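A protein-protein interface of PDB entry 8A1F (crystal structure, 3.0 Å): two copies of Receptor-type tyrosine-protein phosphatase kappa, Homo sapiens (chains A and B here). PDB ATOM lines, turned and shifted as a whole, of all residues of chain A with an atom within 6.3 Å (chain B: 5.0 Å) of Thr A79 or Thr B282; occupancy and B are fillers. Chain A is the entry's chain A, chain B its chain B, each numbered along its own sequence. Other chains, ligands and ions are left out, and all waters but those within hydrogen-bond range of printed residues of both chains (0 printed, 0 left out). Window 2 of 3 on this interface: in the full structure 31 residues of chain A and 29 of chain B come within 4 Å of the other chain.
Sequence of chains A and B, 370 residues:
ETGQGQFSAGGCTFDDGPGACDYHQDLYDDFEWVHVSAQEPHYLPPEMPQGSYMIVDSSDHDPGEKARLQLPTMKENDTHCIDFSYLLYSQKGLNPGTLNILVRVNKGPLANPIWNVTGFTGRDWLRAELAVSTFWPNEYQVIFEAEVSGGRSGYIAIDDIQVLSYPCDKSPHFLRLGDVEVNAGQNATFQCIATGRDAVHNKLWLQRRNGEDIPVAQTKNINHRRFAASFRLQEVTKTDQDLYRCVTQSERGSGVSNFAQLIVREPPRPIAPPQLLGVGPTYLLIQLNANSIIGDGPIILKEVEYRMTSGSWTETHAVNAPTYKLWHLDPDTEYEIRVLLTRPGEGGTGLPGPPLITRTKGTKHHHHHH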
ATOM      1  N   ASN A  77       2.895   8.718   1.400  1.00  0.00           N
ATOM      2  CA  ASN A  77       3.063   7.322   1.802  1.00  0.00           C
ATOM      3  C   ASN A  77       1.987   6.796   2.749  1.00  0.00           C
ATOM      4  O   ASN A  77       1.593   5.631   2.628  1.00  0.00           O
ATOM      5  CB  ASN A  77       4.433   7.118   2.459  1.00  0.00           C
ATOM      6  CG  ASN A  77       5.577   7.392   1.508  1.00  0.00           C
ATOM      7  OD1 ASN A  77       5.723   6.702   0.503  1.00  0.00           O
ATOM      8  ND2 ASN A  77       6.386   8.403   1.806  1.00  0.00           N
ATOM      9  N   ASP A  78       1.506   7.600   3.690  1.00  0.00           N
ATOM     10  CA  ASP A  78       0.536   7.129   4.670  1.00  0.00           C
ATOM     11  C   ASP A  78      -0.899   7.365   4.205  1.00  0.00           C
ATOM     12  O   ASP A  78      -1.194   8.330   3.496  1.00  0.00           O
ATOM     13  CB  ASP A  78       0.775   7.804   6.024  1.00  0.00           C
ATOM     14  CG  ASP A  78       2.029   7.292   6.714  1.00  0.00           C
ATOM     15  OD1 ASP A  78       2.859   6.656   6.030  1.00  0.00           O
ATOM     16  OD2 ASP A  78       2.179   7.514   7.936  1.00  0.00           O
ATOM     17  N   THR A  79      -1.785   6.447   4.596  1.00  0.00           N
ATOM     18  CA  THR A  79      -3.207   6.566   4.288  1.00  0.00           C
ATOM     19  C   THR A  79      -3.759   7.915   4.735  1.00  0.00           C
ATOM     20  O   THR A  79      -3.436   8.413   5.816  1.00  0.00           O
ATOM     21  CB  THR A  79      -3.992   5.431   4.951  1.00  0.00           C
ATOM     22  OG1 THR A  79      -3.943   5.578   6.373  1.00  0.00           O
ATOM     23  CG2 THR A  79      -3.395   4.090   4.564  1.00  0.00           C
ATOM     24  N   HIS A  80      -4.608   8.498   3.892  1.00  0.00           N
ATOM     25  CA  HIS A  80      -5.162   9.827   4.118  1.00  0.00           C
ATOM     26  C   HIS A  80      -6.458   9.969   3.331  1.00  0.00           C
ATOM     27  O   HIS A  80      -6.809   9.113   2.514  1.00  0.00           O
ATOM     28  CB  HIS A  80      -4.163  10.906   3.709  1.00  0.00           C
ATOM     29  CG  HIS A  80      -3.794  10.848   2.260  1.00  0.00           C
ATOM     30  ND1 HIS A  80      -2.877   9.944   1.767  1.00  0.00           N
ATOM     31  CD2 HIS A  80      -4.228  11.564   1.196  1.00  0.00           C
ATOM     32  CE1 HIS A  80      -2.755  10.114   0.463  1.00  0.00           C
ATOM     33  NE2 HIS A  80      -3.563  11.090   0.091  1.00  0.00           N
ATOM     34  N   CYS A  81      -7.168  11.068   3.588  1.00  0.00           N
ATOM     35  CA  CYS A  81      -8.434  11.341   2.923  1.00  0.00           C
ATOM     36  C   CYS A  81      -8.580  12.840   2.692  1.00  0.00           C
ATOM     37  O   CYS A  81      -7.890  13.658   3.307  1.00  0.00           O
ATOM     38  CB  CYS A  81      -9.635  10.827   3.734  1.00  0.00           C
ATOM     39  SG  CYS A  81      -9.835  11.575   5.368  1.00  0.00           S
ATOM     40  N   PHE A 135      -0.352   5.972  -3.702  1.00  0.00           N
ATOM     41  CA  PHE A 135       0.732   6.292  -2.790  1.00  0.00           C
ATOM     42  C   PHE A 135       2.065   6.347  -3.528  1.00  0.00           C
ATOM     43  O   PHE A 135       2.217   5.824  -4.634  1.00  0.00           O
ATOM     44  CB  PHE A 135       0.809   5.276  -1.641  1.00  0.00           C
ATOM     45  CG  PHE A 135      -0.462   5.164  -0.847  1.00  0.00           C
ATOM     46  CD1 PHE A 135      -0.902   6.220  -0.065  1.00  0.00           C
ATOM     47  CD2 PHE A 135      -1.212   4.001  -0.875  1.00  0.00           C
ATOM     48  CE1 PHE A 135      -2.073   6.119   0.666  1.00  0.00           C
ATOM     49  CE2 PHE A 135      -2.380   3.893  -0.146  1.00  0.00           C
ATOM     50  CZ  PHE A 135      -2.812   4.952   0.626  1.00  0.00           C
ATOM     51  N   LEU A 164      -6.685  15.071   5.350  1.00  0.00           N
ATOM     52  CA  LEU A 164      -6.714  14.597   6.726  1.00  0.00           C
ATOM     53  C   LEU A 164      -6.094  13.213   6.848  1.00  0.00           C
ATOM     54  O   LEU A 164      -6.194  12.385   5.938  1.00  0.00           O
ATOM     55  CB  LEU A 164      -8.150  14.555   7.261  1.00  0.00           C
ATOM     56  CG  LEU A 164      -8.899  15.888   7.259  1.00  0.00           C
ATOM     57  CD1 LEU A 164     -10.333  15.687   7.721  1.00  0.00           C
ATOM     58  CD2 LEU A 164      -8.181  16.917   8.124  1.00  0.00           C
ATOM     59  N   SER A 165      -5.441  12.976   7.989  1.00  0.00           N
ATOM     60  CA  SER A 165      -4.933  11.655   8.332  1.00  0.00           C
ATOM     61  C   SER A 165      -5.856  10.878   9.263  1.00  0.00           C
ATOM     62  O   SER A 165      -5.786   9.644   9.284  1.00  0.00           O
ATOM     63  CB  SER A 165      -3.548  11.765   8.980  1.00  0.00           C
ATOM     64  OG  SER A 165      -2.663  12.523   8.172  1.00  0.00           O
ATOM     65  N   TYR A 166      -6.714  11.559  10.020  1.00  0.00           N
ATOM     66  CA  TYR A 166      -7.692  10.884  10.864  1.00  0.00           C
ATOM     67  C   TYR A 166      -8.901  11.796  10.980  1.00  0.00           C
ATOM     68  O   TYR A 166      -8.763  13.020  10.860  1.00  0.00           O
ATOM     69  CB  TYR A 166      -7.152  10.569  12.270  1.00  0.00           C
ATOM     70  CG  TYR A 166      -6.769  11.777  13.095  1.00  0.00           C
ATOM     71  CD1 TYR A 166      -5.522  12.373  12.970  1.00  0.00           C
ATOM     72  CD2 TYR A 166      -7.660  12.305  14.023  1.00  0.00           C
ATOM     73  CE1 TYR A 166      -5.179  13.471  13.740  1.00  0.00           C
ATOM     74  CE2 TYR A 166      -7.329  13.396  14.791  1.00  0.00           C
ATOM     75  CZ  TYR A 166      -6.089  13.976  14.648  1.00  0.00           C
ATOM     76  OH  TYR A 166      -5.772  15.066  15.422  1.00  0.00           O
ATOM     77  N   CYS A 168     -10.931   9.866   8.948  1.00  0.00           N
ATOM     78  CA  CYS A 168     -11.153   9.315   7.612  1.00  0.00           C
ATOM     79  C   CYS A 168     -12.064   8.089   7.679  1.00  0.00           C
ATOM     80  O   CYS A 168     -11.701   6.977   7.291  1.00  0.00           O
ATOM     81  CB  CYS A 168      -9.827   8.980   6.922  1.00  0.00           C
ATOM     82  SG  CYS A 168      -8.746  10.395   6.610  1.00  0.00           S
ATOM     83  N   GLY B 280       2.751   1.096  10.195  1.00  0.00           N
ATOM     84  CA  GLY B 280       1.950   2.176  10.714  1.00  0.00           C
ATOM     85  C   GLY B 280       0.681   1.617  11.316  1.00  0.00           C
ATOM     86  O   GLY B 280       0.523   0.399  11.451  1.00  0.00           O
ATOM     87  N   PRO B 281      -0.250   2.491  11.704  1.00  0.00           N
ATOM     88  CA  PRO B 281      -1.546   1.992  12.185  1.00  0.00           C
ATOM     89  C   PRO B 281      -2.314   1.207  11.138  1.00  0.00           C
ATOM     90  O   PRO B 281      -3.073   0.298  11.496  1.00  0.00           O
ATOM     91  CB  PRO B 281      -2.290   3.274  12.582  1.00  0.00           C
ATOM     92  CG  PRO B 281      -1.212   4.269  12.852  1.00  0.00           C
ATOM     93  CD  PRO B 281      -0.128   3.949  11.861  1.00  0.00           C
ATOM     94  N   THR B 282      -2.145   1.521   9.851  1.00  0.00           N
ATOM     95  CA  THR B 282      -2.948   0.896   8.805  1.00  0.00           C
ATOM     96  C   THR B 282      -2.129   0.332   7.648  1.00  0.00           C
ATOM     97  O   THR B 282      -2.709   0.011   6.603  1.00  0.00           O
ATOM     98  CB  THR B 282      -3.980   1.890   8.255  1.00  0.00           C
ATOM     99  OG1 THR B 282      -3.309   3.036   7.725  1.00  0.00           O
ATOM    100  CG2 THR B 282      -4.953   2.329   9.347  1.00  0.00           C
ATOM    101  N   TYR B 283      -0.810   0.202   7.788  1.00  0.00           N
ATOM    102  CA  TYR B 283      -0.002  -0.326   6.698  1.00  0.00           C
ATOM    103  C   TYR B 283       1.149  -1.172   7.226  1.00  0.00           C
ATOM    104  O   TYR B 283       1.604  -1.002   8.360  1.00  0.00           O
ATOM    105  CB  TYR B 283       0.538   0.799   5.794  1.00  0.00           C
ATOM    106  CG  TYR B 283       1.731   1.563   6.328  1.00  0.00           C
ATOM    107  CD1 TYR B 283       3.030   1.099   6.137  1.00  0.00           C
ATOM    108  CD2 TYR B 283       1.560   2.770   6.993  1.00  0.00           C
ATOM    109  CE1 TYR B 283       4.119   1.802   6.618  1.00  0.00           C
ATOM    110  CE2 TYR B 283       2.641   3.481   7.472  1.00  0.00           C
ATOM    111  CZ  TYR B 283       3.918   2.992   7.284  1.00  0.00           C
ATOM    112  OH  TYR B 283       5.001   3.692   7.758  1.00  0.00           O
ATOM    113  N   LEU B 284       1.605  -2.096   6.377  1.00  0.00           N
ATOM    114  CA  LEU B 284       2.808  -2.889   6.602  1.00  0.00           C
ATOM    115  C   LEU B 284       3.672  -2.845   5.349  1.00  0.00           C
ATOM    116  O   LEU B 284       3.171  -3.052   4.238  1.00  0.00           O
ATOM    117  CB  LEU B 284       2.471  -4.346   6.955  1.00  0.00           C
ATOM    118  CG  LEU B 284       1.772  -4.637   8.286  1.00  0.00           C
ATOM    119  CD1 LEU B 284       1.230  -6.059   8.299  1.00  0.00           C
ATOM    120  CD2 LEU B 284       2.715  -4.416   9.459  1.00  0.00           C
ATOM    121  N   LEU B 326       1.372  -3.243   2.064  1.00  0.00           N
ATOM    122  CA  LEU B 326      -0.037  -3.521   2.299  1.00  0.00           C
ATOM    123  C   LEU B 326      -0.625  -2.341   3.056  1.00  0.00           C
ATOM    124  O   LEU B 326       0.041  -1.780   3.929  1.00  0.00           O
ATOM    125  CB  LEU B 326      -0.209  -4.798   3.119  1.00  0.00           C
ATOM    126  CG  LEU B 326       0.534  -6.019   2.586  1.00  0.00           C
ATOM    127  CD1 LEU B 326       0.380  -7.196   3.533  1.00  0.00           C
ATOM    128  CD2 LEU B 326       0.058  -6.389   1.191  1.00  0.00           C
ATOM    129  N   TRP B 327      -1.863  -1.952   2.736  1.00  0.00           N
ATOM    130  CA  TRP B 327      -2.399  -0.717   3.295  1.00  0.00           C
ATOM    131  C   TRP B 327      -3.889  -0.844   3.582  1.00  0.00           C
ATOM    132  O   TRP B 327      -4.563  -1.785   3.150  1.00  0.00           O
ATOM    133  CB  TRP B 327      -2.133   0.488   2.374  1.00  0.00           C
ATOM    134  CG  TRP B 327      -2.594   0.342   0.937  1.00  0.00           C
ATOM    135  CD1 TRP B 327      -3.873   0.139   0.496  1.00  0.00           C
ATOM    136  CD2 TRP B 327      -1.772   0.406  -0.238  1.00  0.00           C
ATOM    137  NE1 TRP B 327      -3.893   0.066  -0.879  1.00  0.00           N
ATOM    138  CE2 TRP B 327      -2.617   0.226  -1.351  1.00  0.00           C
ATOM    139  CE3 TRP B 327      -0.403   0.592  -0.455  1.00  0.00           C
ATOM    140  CZ2 TRP B 327      -2.137   0.229  -2.664  1.00  0.00           C
ATOM    141  CZ3 TRP B 327       0.071   0.595  -1.758  1.00  0.00           C
ATOM    142  CH2 TRP B 327      -0.793   0.414  -2.843  1.00  0.00           C
ATOM    143  N   HIS B 328      -4.383   0.140   4.340  1.00  0.00           N
ATOM    144  CA  HIS B 328      -5.727   0.140   4.923  1.00  0.00           C
ATOM    145  C   HIS B 328      -6.003  -1.123   5.739  1.00  0.00           C
ATOM    146  O   HIS B 328      -7.107  -1.668   5.732  1.00  0.00           O
ATOM    147  CB  HIS B 328      -6.780   0.359   3.841  1.00  0.00           C
ATOM    148  CG  HIS B 328      -6.780   1.754   3.299  1.00  0.00           C
ATOM    149  ND1 HIS B 328      -6.745   2.038   1.951  1.00  0.00           N
ATOM    150  CD2 HIS B 328      -6.792   2.950   3.935  1.00  0.00           C
ATOM    151  CE1 HIS B 328      -6.742   3.347   1.780  1.00  0.00           C
ATOM    152  NE2 HIS B 328      -6.769   3.924   2.968  1.00  0.00           N
ATOM    153  N   LEU B 329      -4.986  -1.581   6.461  1.00  0.00           N
ATOM    154  CA  LEU B 329      -5.128  -2.618   7.468  1.00  0.00           C
ATOM    155  C   LEU B 329      -5.723  -2.026   8.744  1.00  0.00           C
ATOM    156  O   LEU B 329      -5.683  -0.816   8.970  1.00  0.00           O
ATOM    157  CB  LEU B 329      -3.767  -3.256   7.753  1.00  0.00           C
ATOM    158  CG  LEU B 329      -3.005  -3.731   6.510  1.00  0.00           C
ATOM    159  CD1 LEU B 329      -1.664  -4.347   6.889  1.00  0.00           C
ATOM    160  CD2 LEU B 329      -3.836  -4.717   5.707  1.00  0.00           C
ATOM    161  N   PRO B 331      -5.818  -1.095  12.662  1.00  0.00           N
ATOM    162  CA  PRO B 331      -4.838  -0.898  13.731  1.00  0.00           C
ATOM    163  C   PRO B 331      -4.919  -1.976  14.803  1.00  0.00           C
ATOM    164  O   PRO B 331      -5.984  -2.530  15.095  1.00  0.00           O
ATOM    165  CB  PRO B 331      -5.210   0.479  14.297  1.00  0.00           C
ATOM    166  CG  PRO B 331      -5.974   1.150  13.200  1.00  0.00           C
ATOM    167  CD  PRO B 331      -6.739   0.045  12.545  1.00  0.00           C
ATOM    168  N   THR B 360      -0.141  -4.287  13.177  1.00  0.00           N
ATOM    169  CA  THR B 360      -0.116  -2.853  12.936  1.00  0.00           C
ATOM    170  C   THR B 360      -0.058  -2.069  14.248  1.00  0.00           C
ATOM    171  O   THR B 360      -0.362  -2.582  15.331  1.00  0.00           O
ATOM    172  CB  THR B 360      -1.345  -2.431  12.127  1.00  0.00           C
ATOM    173  OG1 THR B 360      -2.516  -3.048  12.672  1.00  0.00           O
ATOM    174  CG2 THR B 360      -1.194  -2.855  10.671  1.00  0.00           C
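OD1 of Asp A78 touches CE2 of Tyr B283 (3.5 Å).
His B328 touches Thr A79.
Trp B327 touches Phe A135 (CE3 to CD2, 3.5 Å).
ND1 of His A80 is in hydrogen-bond range of O of Asp A78 (2.9 Å).
The backbone carbonyl oxygen of Thr B282 sits at hydrogen-bond distance from the backbone NH of His B328.
The backbone carbonyl oxygen (O) of Thr B282 is in hydrogen-bond range of the backbone NH (N) of Leu B329 (2.8 Å).
The side-chain sulfur (SG) of Cys A168 forms a disulfide with the side-chain sulfur (SG) of Cys A81, 2.0 Å away.
No position is printed for both chains.
The side-chain hydroxyl of Thr A79 sits at hydrogen-bond distance from the side-chain hydroxyl of Thr B282, at 2.9 Å.
Of the 10 printed residues of chain A, 3 touch a printed residue of chain B.
Hydrophobic or aromatic side chains of chain A that line the printed part of chain B: Phe A135.
Printed residues of chain B that touch a printed residue of chain A: Thr B282, Tyr B283, Trp B327 and His B328.
Hydrophobic or aromatic side chains of chain B within 4 Å of the printed part of chain A: Tyr B283, Trp B327 and His B328.
Of chain B, only Thr B282 and His B328 come within 4 Å of Thr A79.
Of chain A, only Thr A79 (2.9 Å) comes within 4 Å of Thr B282.
Of the printed residues of chain B, Asp A78 touches Tyr B283.
Of the printed residues of chain A, Tyr B283 touches Asp A78.
Of the printed residues of chain A, Trp B327 touches Phe A135.
The nearest residue of chain B that does not touch Thr A79 is Trp B327 (4.4 Å).
The nearest printed residue of chain B that does not touch Asp A78 is Pro B281 (5.8 Å).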
